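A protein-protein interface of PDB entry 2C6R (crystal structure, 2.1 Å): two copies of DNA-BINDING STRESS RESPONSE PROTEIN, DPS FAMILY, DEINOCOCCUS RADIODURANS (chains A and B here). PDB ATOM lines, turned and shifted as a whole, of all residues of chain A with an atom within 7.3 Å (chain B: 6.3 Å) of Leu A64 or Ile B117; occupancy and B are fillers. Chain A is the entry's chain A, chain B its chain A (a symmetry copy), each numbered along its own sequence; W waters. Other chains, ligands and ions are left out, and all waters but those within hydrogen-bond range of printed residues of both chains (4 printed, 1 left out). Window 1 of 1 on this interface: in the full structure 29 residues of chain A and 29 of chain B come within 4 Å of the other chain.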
ATOM      1  N   GLU A  58      25.331  15.224  -9.273  1.00  0.00           N
ATOM      2  CA  GLU A  58      23.973  15.617  -9.608  1.00  0.00           C
ATOM      3  C   GLU A  58      23.092  14.396  -9.879  1.00  0.00           C
ATOM      4  O   GLU A  58      21.908  14.391  -9.533  1.00  0.00           O
ATOM      5  CB  GLU A  58      23.969  16.550 -10.820  1.00  0.00           C
ATOM      6  CG  GLU A  58      24.575  17.924 -10.444  1.00  0.00           C
ATOM      7  CD  GLU A  58      24.779  18.873 -11.616  1.00  0.00           C
ATOM      8  OE1 GLU A  58      24.685  18.467 -12.793  1.00  0.00           O
ATOM      9  OE2 GLU A  58      25.065  20.059 -11.343  1.00  0.00           O
ATOM     10  N   LEU A  59      23.658  13.376 -10.509  1.00  0.00           N
ATOM     11  CA  LEU A  59      22.852  12.177 -10.813  1.00  0.00           C
ATOM     12  C   LEU A  59      22.562  11.440  -9.520  1.00  0.00           C
ATOM     13  O   LEU A  59      21.457  10.946  -9.312  1.00  0.00           O
ATOM     14  CB  LEU A  59      23.588  11.277 -11.831  1.00  0.00           C
ATOM     15  CG  LEU A  59      23.620  11.915 -13.220  1.00  0.00           C
ATOM     16  CD1 LEU A  59      24.618  11.171 -14.106  1.00  0.00           C
ATOM     17  CD2 LEU A  59      22.227  12.039 -13.881  1.00  0.00           C
ATOM     18  N   GLN A  60      23.554  11.374  -8.647  1.00  0.00           N
ATOM     19  CA  GLN A  60      23.357  10.716  -7.348  1.00  0.00           C
ATOM     20  C   GLN A  60      22.339  11.416  -6.459  1.00  0.00           C
ATOM     21  O   GLN A  60      21.564  10.749  -5.749  1.00  0.00           O
ATOM     22  CB  GLN A  60      24.658  10.596  -6.616  1.00  0.00           C
ATOM     23  CG  GLN A  60      25.619   9.613  -7.172  1.00  0.00           C
ATOM     24  CD  GLN A  60      26.785   9.463  -6.215  1.00  0.00           C
ATOM     25  OE1 GLN A  60      27.592  10.372  -6.082  1.00  0.00           O
ATOM     26  NE2 GLN A  60      26.835   8.352  -5.499  1.00  0.00           N
ATOM     27  N   ALA A  61      22.347  12.755  -6.492  1.00  0.00           N
ATOM     28  CA  ALA A  61      21.322  13.570  -5.828  1.00  0.00           C
ATOM     29  C   ALA A  61      19.957  13.197  -6.395  1.00  0.00           C
ATOM     30  O   ALA A  61      19.017  12.988  -5.653  1.00  0.00           O
ATOM     31  CB  ALA A  61      21.593  15.097  -6.066  1.00  0.00           C
ATOM     32  N   LEU A  62      19.862  13.129  -7.719  1.00  0.00           N
ATOM     33  CA  LEU A  62      18.637  12.710  -8.402  1.00  0.00           C
ATOM     34  C   LEU A  62      18.213  11.263  -8.079  1.00  0.00           C
ATOM     35  O   LEU A  62      17.038  11.021  -7.892  1.00  0.00           O
ATOM     36  CB  LEU A  62      18.744  12.956  -9.933  1.00  0.00           C
ATOM     37  CG  LEU A  62      18.572  14.422 -10.405  1.00  0.00           C
ATOM     38  CD1 LEU A  62      18.906  14.564 -11.871  1.00  0.00           C
ATOM     39  CD2 LEU A  62      17.172  15.036 -10.137  1.00  0.00           C
ATOM     40  N   GLN A  63      19.153  10.318  -8.014  1.00  0.00           N
ATOM     41  CA  GLN A  63      18.834   8.965  -7.501  1.00  0.00           C
ATOM     42  C   GLN A  63      18.102   9.022  -6.171  1.00  0.00           C
ATOM     43  O   GLN A  63      17.003   8.478  -6.020  1.00  0.00           O
ATOM     44  CB  GLN A  63      20.095   8.129  -7.286  1.00  0.00           C
ATOM     45  CG  GLN A  63      20.721   7.561  -8.526  1.00  0.00           C
ATOM     46  CD  GLN A  63      21.907   6.712  -8.169  1.00  0.00           C
ATOM     47  OE1 GLN A  63      22.993   7.220  -7.800  1.00  0.00           O
ATOM     48  NE2 GLN A  63      21.747   5.413  -8.336  1.00  0.00           N
ATOM     49  N   LEU A  64      18.712   9.700  -5.193  1.00  0.00           N
ATOM     50  CA  LEU A  64      18.065   9.832  -3.885  1.00  0.00           C
ATOM     51  C   LEU A  64      16.727  10.560  -3.912  1.00  0.00           C
ATOM     52  O   LEU A  64      15.789  10.164  -3.222  1.00  0.00           O
ATOM     53  CB  LEU A  64      19.022  10.477  -2.848  1.00  0.00           C
ATOM     54  CG  LEU A  64      20.320   9.741  -2.599  1.00  0.00           C
ATOM     55  CD1 LEU A  64      21.329  10.654  -1.852  1.00  0.00           C
ATOM     56  CD2 LEU A  64      20.105   8.434  -1.848  1.00  0.00           C
ATOM     57  N   GLN A  65      16.607  11.627  -4.702  1.00  0.00           N
ATOM     58  CA  GLN A  65      15.324  12.336  -4.694  1.00  0.00           C
ATOM     59  C   GLN A  65      14.204  11.558  -5.415  1.00  0.00           C
ATOM     60  O   GLN A  65      13.069  11.556  -4.974  1.00  0.00           O
ATOM     61  CB  GLN A  65      15.466  13.741  -5.297  1.00  0.00           C
ATOM     62  CG  GLN A  65      16.341  14.670  -4.415  1.00  0.00           C
ATOM     63  CD  GLN A  65      16.991  15.777  -5.221  1.00  0.00           C
ATOM     64  OE1 GLN A  65      16.885  15.802  -6.446  1.00  0.00           O
ATOM     65  NE2 GLN A  65      17.688  16.694  -4.533  1.00  0.00           N
ATOM     66  N   THR A  66      14.525  10.933  -6.542  1.00  0.00           N
ATOM     67  CA  THR A  66      13.490  10.124  -7.251  1.00  0.00           C
ATOM     68  C   THR A  66      12.973   8.961  -6.373  1.00  0.00           C
ATOM     69  O   THR A  66      11.754   8.723  -6.311  1.00  0.00           O
ATOM     70  CB  THR A  66      13.966   9.565  -8.639  1.00  0.00           C
ATOM     71  OG1 THR A  66      15.172   8.817  -8.470  1.00  0.00           O
ATOM     72  CG2 THR A  66      14.200  10.691  -9.612  1.00  0.00           C
ATOM     73  N   LYS A  67      13.881   8.240  -5.714  1.00  0.00           N
ATOM     74  CA  LYS A  67      13.469   7.158  -4.824  1.00  0.00           C
ATOM     75  C   LYS A  67      12.598   7.703  -3.691  1.00  0.00           C
ATOM     76  O   LYS A  67      11.570   7.117  -3.352  1.00  0.00           O
ATOM     77  CB  LYS A  67      14.670   6.488  -4.154  1.00  0.00           C
ATOM     78  CG  LYS A  67      15.116   5.164  -4.717  1.00  0.00           C
ATOM     79  CD  LYS A  67      14.013   4.152  -4.959  1.00  0.00           C
ATOM     80  CE  LYS A  67      14.625   2.999  -5.695  1.00  0.00           C
ATOM     81  NZ  LYS A  67      13.701   1.893  -5.683  1.00  0.00           N
ATOM     82  N   GLN A  68      13.053   8.796  -3.069  1.00  0.00           N
ATOM     83  CA  GLN A  68      12.312   9.400  -1.964  1.00  0.00           C
ATOM     84  C   GLN A  68      10.872   9.699  -2.390  1.00  0.00           C
ATOM     85  O   GLN A  68       9.925   9.367  -1.682  1.00  0.00           O
ATOM     86  CB  GLN A  68      12.980  10.694  -1.536  1.00  0.00           C
ATOM     87  CG  GLN A  68      12.185  11.543  -0.490  1.00  0.00           C
ATOM     88  CD  GLN A  68      12.502  11.125   0.902  1.00  0.00           C
ATOM     89  OE1 GLN A  68      13.346  10.266   1.108  1.00  0.00           O
ATOM     90  NE2 GLN A  68      11.813  11.715   1.885  1.00  0.00           N
ATOM     91  N   ALA A  69      10.739  10.323  -3.555  1.00  0.00           N
ATOM     92  CA  ALA A  69       9.441  10.657  -4.144  1.00  0.00           C
ATOM     93  C   ALA A  69       8.662   9.383  -4.516  1.00  0.00           C
ATOM     94  O   ALA A  69       7.472   9.281  -4.263  1.00  0.00           O
ATOM     95  CB  ALA A  69       9.640  11.563  -5.361  1.00  0.00           C
ATOM     96  N   HIS A  70       9.365   8.393  -5.068  1.00  0.00           N
ATOM     97  CA  HIS A  70       8.791   7.063  -5.386  1.00  0.00           C
ATOM     98  C   HIS A  70       8.059   6.492  -4.163  1.00  0.00           C
ATOM     99  O   HIS A  70       6.899   6.035  -4.265  1.00  0.00           O
ATOM    100  CB  HIS A  70       9.962   6.158  -5.861  1.00  0.00           C
ATOM    101  CG  HIS A  70       9.639   4.704  -5.991  1.00  0.00           C
ATOM    102  ND1 HIS A  70       8.930   4.188  -7.056  1.00  0.00           N
ATOM    103  CD2 HIS A  70      10.014   3.643  -5.244  1.00  0.00           C
ATOM    104  CE1 HIS A  70       8.834   2.878  -6.932  1.00  0.00           C
ATOM    105  NE2 HIS A  70       9.498   2.519  -5.850  1.00  0.00           N
ATOM    106  N   TRP A  71       8.733   6.527  -3.003  1.00  0.00           N
ATOM    107  CA  TRP A  71       8.131   6.034  -1.749  1.00  0.00           C
ATOM    108  C   TRP A  71       6.983   6.883  -1.182  1.00  0.00           C
ATOM    109  O   TRP A  71       5.970   6.336  -0.728  1.00  0.00           O
ATOM    110  CB  TRP A  71       9.201   5.809  -0.658  1.00  0.00           C
ATOM    111  CG  TRP A  71      10.317   4.839  -1.025  1.00  0.00           C
ATOM    112  CD1 TRP A  71      10.199   3.633  -1.671  1.00  0.00           C
ATOM    113  CD2 TRP A  71      11.717   4.992  -0.712  1.00  0.00           C
ATOM    114  NE1 TRP A  71      11.425   3.054  -1.822  1.00  0.00           N
ATOM    115  CE2 TRP A  71      12.380   3.853  -1.229  1.00  0.00           C
ATOM    116  CE3 TRP A  71      12.466   5.983  -0.024  1.00  0.00           C
ATOM    117  CZ2 TRP A  71      13.781   3.663  -1.097  1.00  0.00           C
ATOM    118  CZ3 TRP A  71      13.874   5.818   0.084  1.00  0.00           C
ATOM    119  CH2 TRP A  71      14.511   4.659  -0.454  1.00  0.00           C
ATOM    120  N   TYR A  89      14.549   6.594 -12.101  1.00  0.00           N
ATOM    121  CA  TYR A  89      15.590   6.159 -11.177  1.00  0.00           C
ATOM    122  C   TYR A  89      16.560   5.156 -11.840  1.00  0.00           C
ATOM    123  O   TYR A  89      17.785   5.280 -11.753  1.00  0.00           O
ATOM    124  CB  TYR A  89      14.937   5.574  -9.920  1.00  0.00           C
ATOM    125  CG  TYR A  89      15.964   5.006  -8.988  1.00  0.00           C
ATOM    126  CD1 TYR A  89      16.613   5.850  -8.066  1.00  0.00           C
ATOM    127  CD2 TYR A  89      16.316   3.650  -9.031  1.00  0.00           C
ATOM    128  CE1 TYR A  89      17.551   5.356  -7.215  1.00  0.00           C
ATOM    129  CE2 TYR A  89      17.299   3.129  -8.161  1.00  0.00           C
ATOM    130  CZ  TYR A  89      17.895   4.006  -7.236  1.00  0.00           C
ATOM    131  OH  TYR A  89      18.883   3.561  -6.357  1.00  0.00           O
ATOM    132  N   ILE A  92      18.628   7.068 -14.585  1.00  0.00           N
ATOM    133  CA  ILE A  92      19.612   7.862 -13.825  1.00  0.00           C
ATOM    134  C   ILE A  92      20.714   7.023 -13.187  1.00  0.00           C
ATOM    135  O   ILE A  92      21.898   7.391 -13.279  1.00  0.00           O
ATOM    136  CB  ILE A  92      18.877   8.719 -12.735  1.00  0.00           C
ATOM    137  CG1 ILE A  92      17.967   9.759 -13.397  1.00  0.00           C
ATOM    138  CG2 ILE A  92      19.888   9.384 -11.735  1.00  0.00           C
ATOM    139  CD1 ILE A  92      16.913  10.295 -12.413  1.00  0.00           C
ATOM    140  N   ALA A 114      28.207  10.027   0.382  1.00  0.00           N
ATOM    141  CA  ALA A 114      27.081  10.775   0.940  1.00  0.00           C
ATOM    142  C   ALA A 114      27.478  12.217   1.308  1.00  0.00           C
ATOM    143  O   ALA A 114      26.747  13.166   0.993  1.00  0.00           O
ATOM    144  CB  ALA A 114      26.537  10.059   2.157  1.00  0.00           C
ATOM    145  N   ILE A 115      28.648  12.369   1.928  1.00  0.00           N
ATOM    146  CA  ILE A 115      29.135  13.699   2.326  1.00  0.00           C
ATOM    147  C   ILE A 115      29.285  14.601   1.105  1.00  0.00           C
ATOM    148  O   ILE A 115      28.847  15.758   1.127  1.00  0.00           O
ATOM    149  CB  ILE A 115      30.429  13.625   3.242  1.00  0.00           C
ATOM    150  CG1 ILE A 115      30.740  15.008   3.856  1.00  0.00           C
ATOM    151  CG2 ILE A 115      31.677  12.995   2.490  1.00  0.00           C
ATOM    152  CD1 ILE A 115      29.653  15.535   4.795  1.00  0.00           C
ATOM    153  N   ILE A 117      27.663  14.355  -1.859  1.00  0.00           N
ATOM    154  CA  ILE A 117      26.316  14.703  -2.282  1.00  0.00           C
ATOM    155  C   ILE A 117      25.746  15.885  -1.468  1.00  0.00           C
ATOM    156  O   ILE A 117      25.288  16.878  -2.045  1.00  0.00           O
ATOM    157  CB  ILE A 117      25.349  13.458  -2.253  1.00  0.00           C
ATOM    158  CG1 ILE A 117      25.880  12.339  -3.193  1.00  0.00           C
ATOM    159  CG2 ILE A 117      23.953  13.890  -2.692  1.00  0.00           C
ATOM    160  CD1 ILE A 117      25.296  10.946  -2.911  1.00  0.00           C
ATOM    161  N   VAL A 118      25.788  15.773  -0.135  1.00  0.00           N
ATOM    162  CA  VAL A 118      25.392  16.898   0.736  1.00  0.00           C
ATOM    163  C   VAL A 118      26.203  18.192   0.455  1.00  0.00           C
ATOM    164  O   VAL A 118      25.618  19.245   0.237  1.00  0.00           O
ATOM    165  CB  VAL A 118      25.401  16.514   2.234  1.00  0.00           C
ATOM    166  CG1 VAL A 118      25.180  17.767   3.107  1.00  0.00           C
ATOM    167  CG2 VAL A 118      24.299  15.507   2.514  1.00  0.00           C
ATOM    168  N   GLU A 125      16.391  21.138  -1.945  1.00  0.00           N
ATOM    169  CA  GLU A 125      16.270  19.798  -1.402  1.00  0.00           C
ATOM    170  C   GLU A 125      14.793  19.390  -1.410  1.00  0.00           C
ATOM    171  O   GLU A 125      13.891  20.240  -1.363  1.00  0.00           O
ATOM    172  CB  GLU A 125      16.969  19.649  -0.041  1.00  0.00           C
ATOM    173  CG  GLU A 125      16.950  18.219   0.592  1.00  0.00           C
ATOM    174  CD  GLU A 125      17.388  17.054  -0.346  1.00  0.00           C
ATOM    175  OE1 GLU A 125      16.976  16.978  -1.544  1.00  0.00           O
ATOM    176  OE2 GLU A 125      18.137  16.177   0.156  1.00  0.00           O
ATOM    177  N   ILE A 126      14.563  18.089  -1.552  1.00  0.00           N
ATOM    178  CA  ILE A 126      13.218  17.527  -1.589  1.00  0.00           C
ATOM    179  C   ILE A 126      12.698  17.514  -0.141  1.00  0.00           C
ATOM    180  O   ILE A 126      13.422  17.120   0.756  1.00  0.00           O
ATOM    181  CB  ILE A 126      13.239  16.086  -2.247  1.00  0.00           C
ATOM    182  CG1 ILE A 126      11.837  15.508  -2.446  1.00  0.00           C
ATOM    183  CG2 ILE A 126      14.100  15.094  -1.444  1.00  0.00           C
ATOM    184  CD1 ILE A 126      11.037  16.209  -3.469  1.00  0.00           C
ATOM    185  N   PHE A 140      10.455  18.058  -9.824  1.00  0.00           N
ATOM    186  CA  PHE A 140      11.322  17.466 -10.852  1.00  0.00           C
ATOM    187  C   PHE A 140      11.329  18.229 -12.145  1.00  0.00           C
ATOM    188  O   PHE A 140      12.346  18.224 -12.828  1.00  0.00           O
ATOM    189  CB  PHE A 140      11.060  15.954 -11.043  1.00  0.00           C
ATOM    190  CG  PHE A 140      11.469  15.139  -9.850  1.00  0.00           C
ATOM    191  CD1 PHE A 140      12.811  14.885  -9.602  1.00  0.00           C
ATOM    192  CD2 PHE A 140      10.527  14.698  -8.937  1.00  0.00           C
ATOM    193  CE1 PHE A 140      13.200  14.168  -8.488  1.00  0.00           C
ATOM    194  CE2 PHE A 140      10.908  13.963  -7.822  1.00  0.00           C
ATOM    195  CZ  PHE A 140      12.234  13.700  -7.588  1.00  0.00           C
ATOM    196  N   THR B  57      18.342   3.680   6.508  1.00  0.00           N
ATOM    197  CA  THR B  57      19.508   4.555   6.421  1.00  0.00           C
ATOM    198  C   THR B  57      20.798   3.789   6.343  1.00  0.00           C
ATOM    199  O   THR B  57      21.683   4.158   5.584  1.00  0.00           O
ATOM    200  CB  THR B  57      19.570   5.547   7.597  1.00  0.00           C
ATOM    201  OG1 THR B  57      18.302   6.182   7.670  1.00  0.00           O
ATOM    202  CG2 THR B  57      20.686   6.621   7.331  1.00  0.00           C
ATOM    203  N   GLN B  60      21.060   2.369   2.857  1.00  0.00           N
ATOM    204  CA  GLN B  60      21.416   3.439   1.914  1.00  0.00           C
ATOM    205  C   GLN B  60      22.872   3.874   2.009  1.00  0.00           C
ATOM    206  O   GLN B  60      23.505   4.173   0.979  1.00  0.00           O
ATOM    207  CB  GLN B  60      20.528   4.629   2.109  1.00  0.00           C
ATOM    208  CG  GLN B  60      19.123   4.458   1.666  1.00  0.00           C
ATOM    209  CD  GLN B  60      18.414   5.797   1.739  1.00  0.00           C
ATOM    210  OE1 GLN B  60      18.149   6.294   2.824  1.00  0.00           O
ATOM    211  NE2 GLN B  60      18.172   6.411   0.592  1.00  0.00           N
ATOM    212  N   ALA B  61      23.396   3.919   3.241  1.00  0.00           N
ATOM    213  CA  ALA B  61      24.826   4.153   3.486  1.00  0.00           C
ATOM    214  C   ALA B  61      25.626   3.062   2.784  1.00  0.00           C
ATOM    215  O   ALA B  61      26.596   3.346   2.107  1.00  0.00           O
ATOM    216  CB  ALA B  61      25.133   4.127   5.024  1.00  0.00           C
ATOM    217  N   GLN B  63      24.568   1.106   0.214  1.00  0.00           N
ATOM    218  CA  GLN B  63      24.469   1.372  -1.240  1.00  0.00           C
ATOM    219  C   GLN B  63      25.577   2.291  -1.724  1.00  0.00           C
ATOM    220  O   GLN B  63      26.337   1.954  -2.638  1.00  0.00           O
ATOM    221  CB  GLN B  63      23.141   2.035  -1.605  1.00  0.00           C
ATOM    222  CG  GLN B  63      21.947   1.127  -1.644  1.00  0.00           C
ATOM    223  CD  GLN B  63      20.728   1.888  -2.077  1.00  0.00           C
ATOM    224  OE1 GLN B  63      20.147   2.693  -1.309  1.00  0.00           O
ATOM    225  NE2 GLN B  63      20.277   1.602  -3.284  1.00  0.00           N
ATOM    226  N   LEU B  64      25.681   3.467  -1.096  1.00  0.00           N
ATOM    227  CA  LEU B  64      26.740   4.405  -1.478  1.00  0.00           C
ATOM    228  C   LEU B  64      28.155   3.877  -1.277  1.00  0.00           C
ATOM    229  O   LEU B  64      29.029   4.105  -2.113  1.00  0.00           O
ATOM    230  CB  LEU B  64      26.559   5.774  -0.769  1.00  0.00           C
ATOM    231  CG  LEU B  64      25.252   6.488  -1.037  1.00  0.00           C
ATOM    232  CD1 LEU B  64      25.034   7.628  -0.007  1.00  0.00           C
ATOM    233  CD2 LEU B  64      25.168   7.017  -2.462  1.00  0.00           C
ATOM    234  N   GLY B 112      14.705   8.906   2.983  1.00  0.00           N
ATOM    235  CA  GLY B 112      15.865   8.467   2.235  1.00  0.00           C
ATOM    236  C   GLY B 112      16.770   9.581   1.734  1.00  0.00           C
ATOM    237  O   GLY B 112      17.572   9.368   0.822  1.00  0.00           O
ATOM    238  N   ARG B 113      16.680  10.769   2.352  1.00  0.00           N
ATOM    239  CA  ARG B 113      17.452  11.934   1.914  1.00  0.00           C
ATOM    240  C   ARG B 113      18.946  11.812   2.230  1.00  0.00           C
ATOM    241  O   ARG B 113      19.338  11.159   3.185  1.00  0.00           O
ATOM    242  CB  ARG B 113      16.846  13.241   2.481  1.00  0.00           C
ATOM    243  CG  ARG B 113      15.425  13.518   1.978  1.00  0.00           C
ATOM    244  CD  ARG B 113      14.717  14.620   2.787  1.00  0.00           C
ATOM    245  NE  ARG B 113      14.618  14.295   4.208  1.00  0.00           N
ATOM    246  CZ  ARG B 113      14.560  15.198   5.186  1.00  0.00           C
ATOM    247  NH1 ARG B 113      14.591  16.486   4.903  1.00  0.00           N
ATOM    248  NH2 ARG B 113      14.461  14.814   6.445  1.00  0.00           N
ATOM    249  N   ALA B 114      19.761  12.423   1.371  1.00  0.00           N
ATOM    250  CA  ALA B 114      21.211  12.516   1.540  1.00  0.00           C
ATOM    251  C   ALA B 114      21.590  13.089   2.918  1.00  0.00           C
ATOM    252  O   ALA B 114      22.481  12.555   3.594  1.00  0.00           O
ATOM    253  CB  ALA B 114      21.807  13.367   0.441  1.00  0.00           C
ATOM    254  N   ILE B 115      20.882  14.138   3.339  1.00  0.00           N
ATOM    255  CA  ILE B 115      21.150  14.769   4.640  1.00  0.00           C
ATOM    256  C   ILE B 115      20.961  13.764   5.772  1.00  0.00           C
ATOM    257  O   ILE B 115      21.807  13.668   6.669  1.00  0.00           O
ATOM    258  CB  ILE B 115      20.350  16.126   4.835  1.00  0.00           C
ATOM    259  CG1 ILE B 115      20.865  16.887   6.078  1.00  0.00           C
ATOM    260  CG2 ILE B 115      18.778  15.913   4.856  1.00  0.00           C
ATOM    261  CD1 ILE B 115      22.326  17.330   5.980  1.00  0.00           C
ATOM    262  N   THR B 116      19.909  12.935   5.667  1.00  0.00           N
ATOM    263  CA  THR B 116      19.624  11.933   6.677  1.00  0.00           C
ATOM    264  C   THR B 116      20.701  10.824   6.753  1.00  0.00           C
ATOM    265  O   THR B 116      21.092  10.378   7.848  1.00  0.00           O
ATOM    266  CB  THR B 116      18.276  11.351   6.381  1.00  0.00           C
ATOM    267  OG1 THR B 116      17.344  12.426   6.217  1.00  0.00           O
ATOM    268  CG2 THR B 116      17.805  10.391   7.467  1.00  0.00           C
ATOM    269  N   ILE B 117      21.188  10.389   5.598  1.00  0.00           N
ATOM    270  CA  ILE B 117      22.317   9.474   5.531  1.00  0.00           C
ATOM    271  C   ILE B 117      23.564  10.049   6.238  1.00  0.00           C
ATOM    272  O   ILE B 117      24.150   9.390   7.105  1.00  0.00           O
ATOM    273  CB  ILE B 117      22.637   9.042   4.049  1.00  0.00           C
ATOM    274  CG1 ILE B 117      21.406   8.341   3.412  1.00  0.00           C
ATOM    275  CG2 ILE B 117      23.838   8.099   4.045  1.00  0.00           C
ATOM    276  CD1 ILE B 117      21.433   8.286   1.876  1.00  0.00           C
ATOM    277  N   VAL B 118      23.951  11.277   5.872  1.00  0.00           N
ATOM    278  CA  VAL B 118      25.048  11.970   6.577  1.00  0.00           C
ATOM    279  C   VAL B 118      24.789  12.112   8.101  1.00  0.00           C
ATOM    280  O   VAL B 118      25.634  11.732   8.903  1.00  0.00           O
ATOM    281  CB  VAL B 118      25.411  13.321   5.916  1.00  0.00           C
ATOM    282  CG1 VAL B 118      26.412  14.095   6.798  1.00  0.00           C
ATOM    283  CG2 VAL B 118      26.031  13.075   4.551  1.00  0.00           C
ATOM    284  N   ALA B 119      23.597  12.579   8.469  1.00  0.00           N
ATOM    285  CA  ALA B 119      23.207  12.739   9.881  1.00  0.00           C
ATOM    286  C   ALA B 119      23.307  11.450  10.712  1.00  0.00           C
ATOM    287  O   ALA B 119      23.594  11.518  11.913  1.00  0.00           O
ATOM    288  CB  ALA B 119      21.825  13.339  10.002  1.00  0.00           C
ATOM    289  N   ALA B 120      23.086  10.284  10.093  1.00  0.00           N
ATOM    290  CA  ALA B 120      23.174   9.011  10.828  1.00  0.00           C
ATOM    291  C   ALA B 120      24.560   8.356  10.783  1.00  0.00           C
ATOM    292  O   ALA B 120      24.694   7.185  11.180  1.00  0.00           O
ATOM    293  CB  ALA B 120      22.117   8.024  10.371  1.00  0.00           C
ATOM    294  N   SER B 121      25.586   9.087  10.331  1.00  0.00           N
ATOM    295  CA  SER B 121      26.936   8.527  10.235  1.00  0.00           C
ATOM    296  C   SER B 121      27.023   7.284  11.119  1.00  0.00           C
ATOM    297  O   SER B 121      26.909   6.143  10.658  1.00  0.00           O
ATOM    298  CB  SER B 121      27.985   9.546  10.683  1.00  0.00           C
ATOM    299  OG  SER B 121      29.118   8.898  11.248  1.00  0.00           O
HETATM  300  O   HOH W   1      17.951  13.825  -1.029  1.00  0.00           O
HETATM  301  O   HOH W   2      14.588  18.219   2.792  1.00  0.00           O
HETATM  302  O   HOH W   3      16.320   8.070  -1.437  1.00  0.00           O
HETATM  303  O   HOH W   4      28.358   5.837  -4.211  1.00  0.00           O
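Gln A60 touches Leu B64, and with the chains exchanged Leu A64 touches Gln B60. Leu A64 touches Ile B117, and with the chains exchanged Ile A117 touches Leu B64. Ala A114 touches Val B118, and with the chains exchanged Val A118 touches Ala B114. Val A118 touches its own counterpart, Val B118. 8 positions are printed for both chains. Of the 20 pairs that touch across the chains among the printed residues, 13 have their exchanged pair printed and touching as well.
CD2 of Leu B64 touches NE2 of Gln A60, at 3.7 Å. CD2 of Leu A64 touches CD1 of Ile B117, 3.96 Å away. Arg B113 touches Gln A68. Trp A71 touches Gly B112. Ala A114 touches Val B118 (O to CG2, 3.6 Å). Leu B64 touches Ile A117. CG2 of Ile A117 touches CB of Ala B114 (3.8 Å). CG2 of Val A118 touches N of Ile B115, at 3.8 Å. Arg B113 touches Glu A125 (CB to OE2, 3.96 Å). Ile A126 touches Arg B113.
Hydrophobic or aromatic side chains of chain B within 4 Å of the printed part of chain A: Leu B64, Ala B114, Ile B117 and Val B118. Printed residues of chain A that touch a printed residue of chain B: Gln A60, Leu A64, Gln A68, Trp A71, Tyr A89, Ala A114, Ile A115, Ile A117, Val A118, Glu A125 and Ile A126. Hydrophobic or aromatic side chains of chain A that line the printed part of chain B: Leu A64, Trp A71, Tyr A89, Ala A114, Ile A117, Val A118 and Ile A126. Among the printed residues, 20 pairs touch across the chains. Among the printed residues, no Asp or Glu carboxylate lies within 4 Å of a Lys or Arg side-chain nitrogen of the other chain.
Water W2 bridges the backbone carbonyl oxygen (O) of Ile A126 (2.6 Å) and the guanidinium group (NH1) of Arg B113 (2.7 Å). Water W1 lies within hydrogen-bond range of OE2 of Glu A125 (2.6 Å) and N of Ala B114 (3.3 Å). Water W3 lies within hydrogen-bond range of the backbone carbonyl oxygen of Leu A64 (2.8 Å), the backbone carbonyl oxygen of Gly B112 (2.9 Å) and the side-chain amide nitrogen of Gln B60 (3.2 Å). Water W4 lies within hydrogen-bond range of O of Leu B64 (2.8 Å) and NE2 of Gln A60 (3.2 Å).
N of Gly B112 is in hydrogen-bond range of OE1 of Gln A68, 2.7 Å away.
The side-chain amide nitrogen of Gln B60 sits at hydrogen-bond distance from the backbone carbonyl oxygen of Gly B112 (3.0 Å). The side-chain amide nitrogen of Gln A65 sits at hydrogen-bond distance from the side-chain carboxylate of Glu A125, at 3.1 Å.
Leu A64 touches just these residues of chain B: Gln B60 (3.7 Å), Gly B112 (3.8 Å), Ala B114 (3.6 Å) and Ile B117 (3.96 Å). His A70 touches none of the printed residues of chain B. Printed residues of chain B within 4 Å of Ala A114: Leu B64, Ile B117 and Val B118. Of the printed residues of chain A, Ile B115 touches Val A118. Thr B116 touches none of the printed residues of chain A. Ile B117 touches two residues of chain A.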
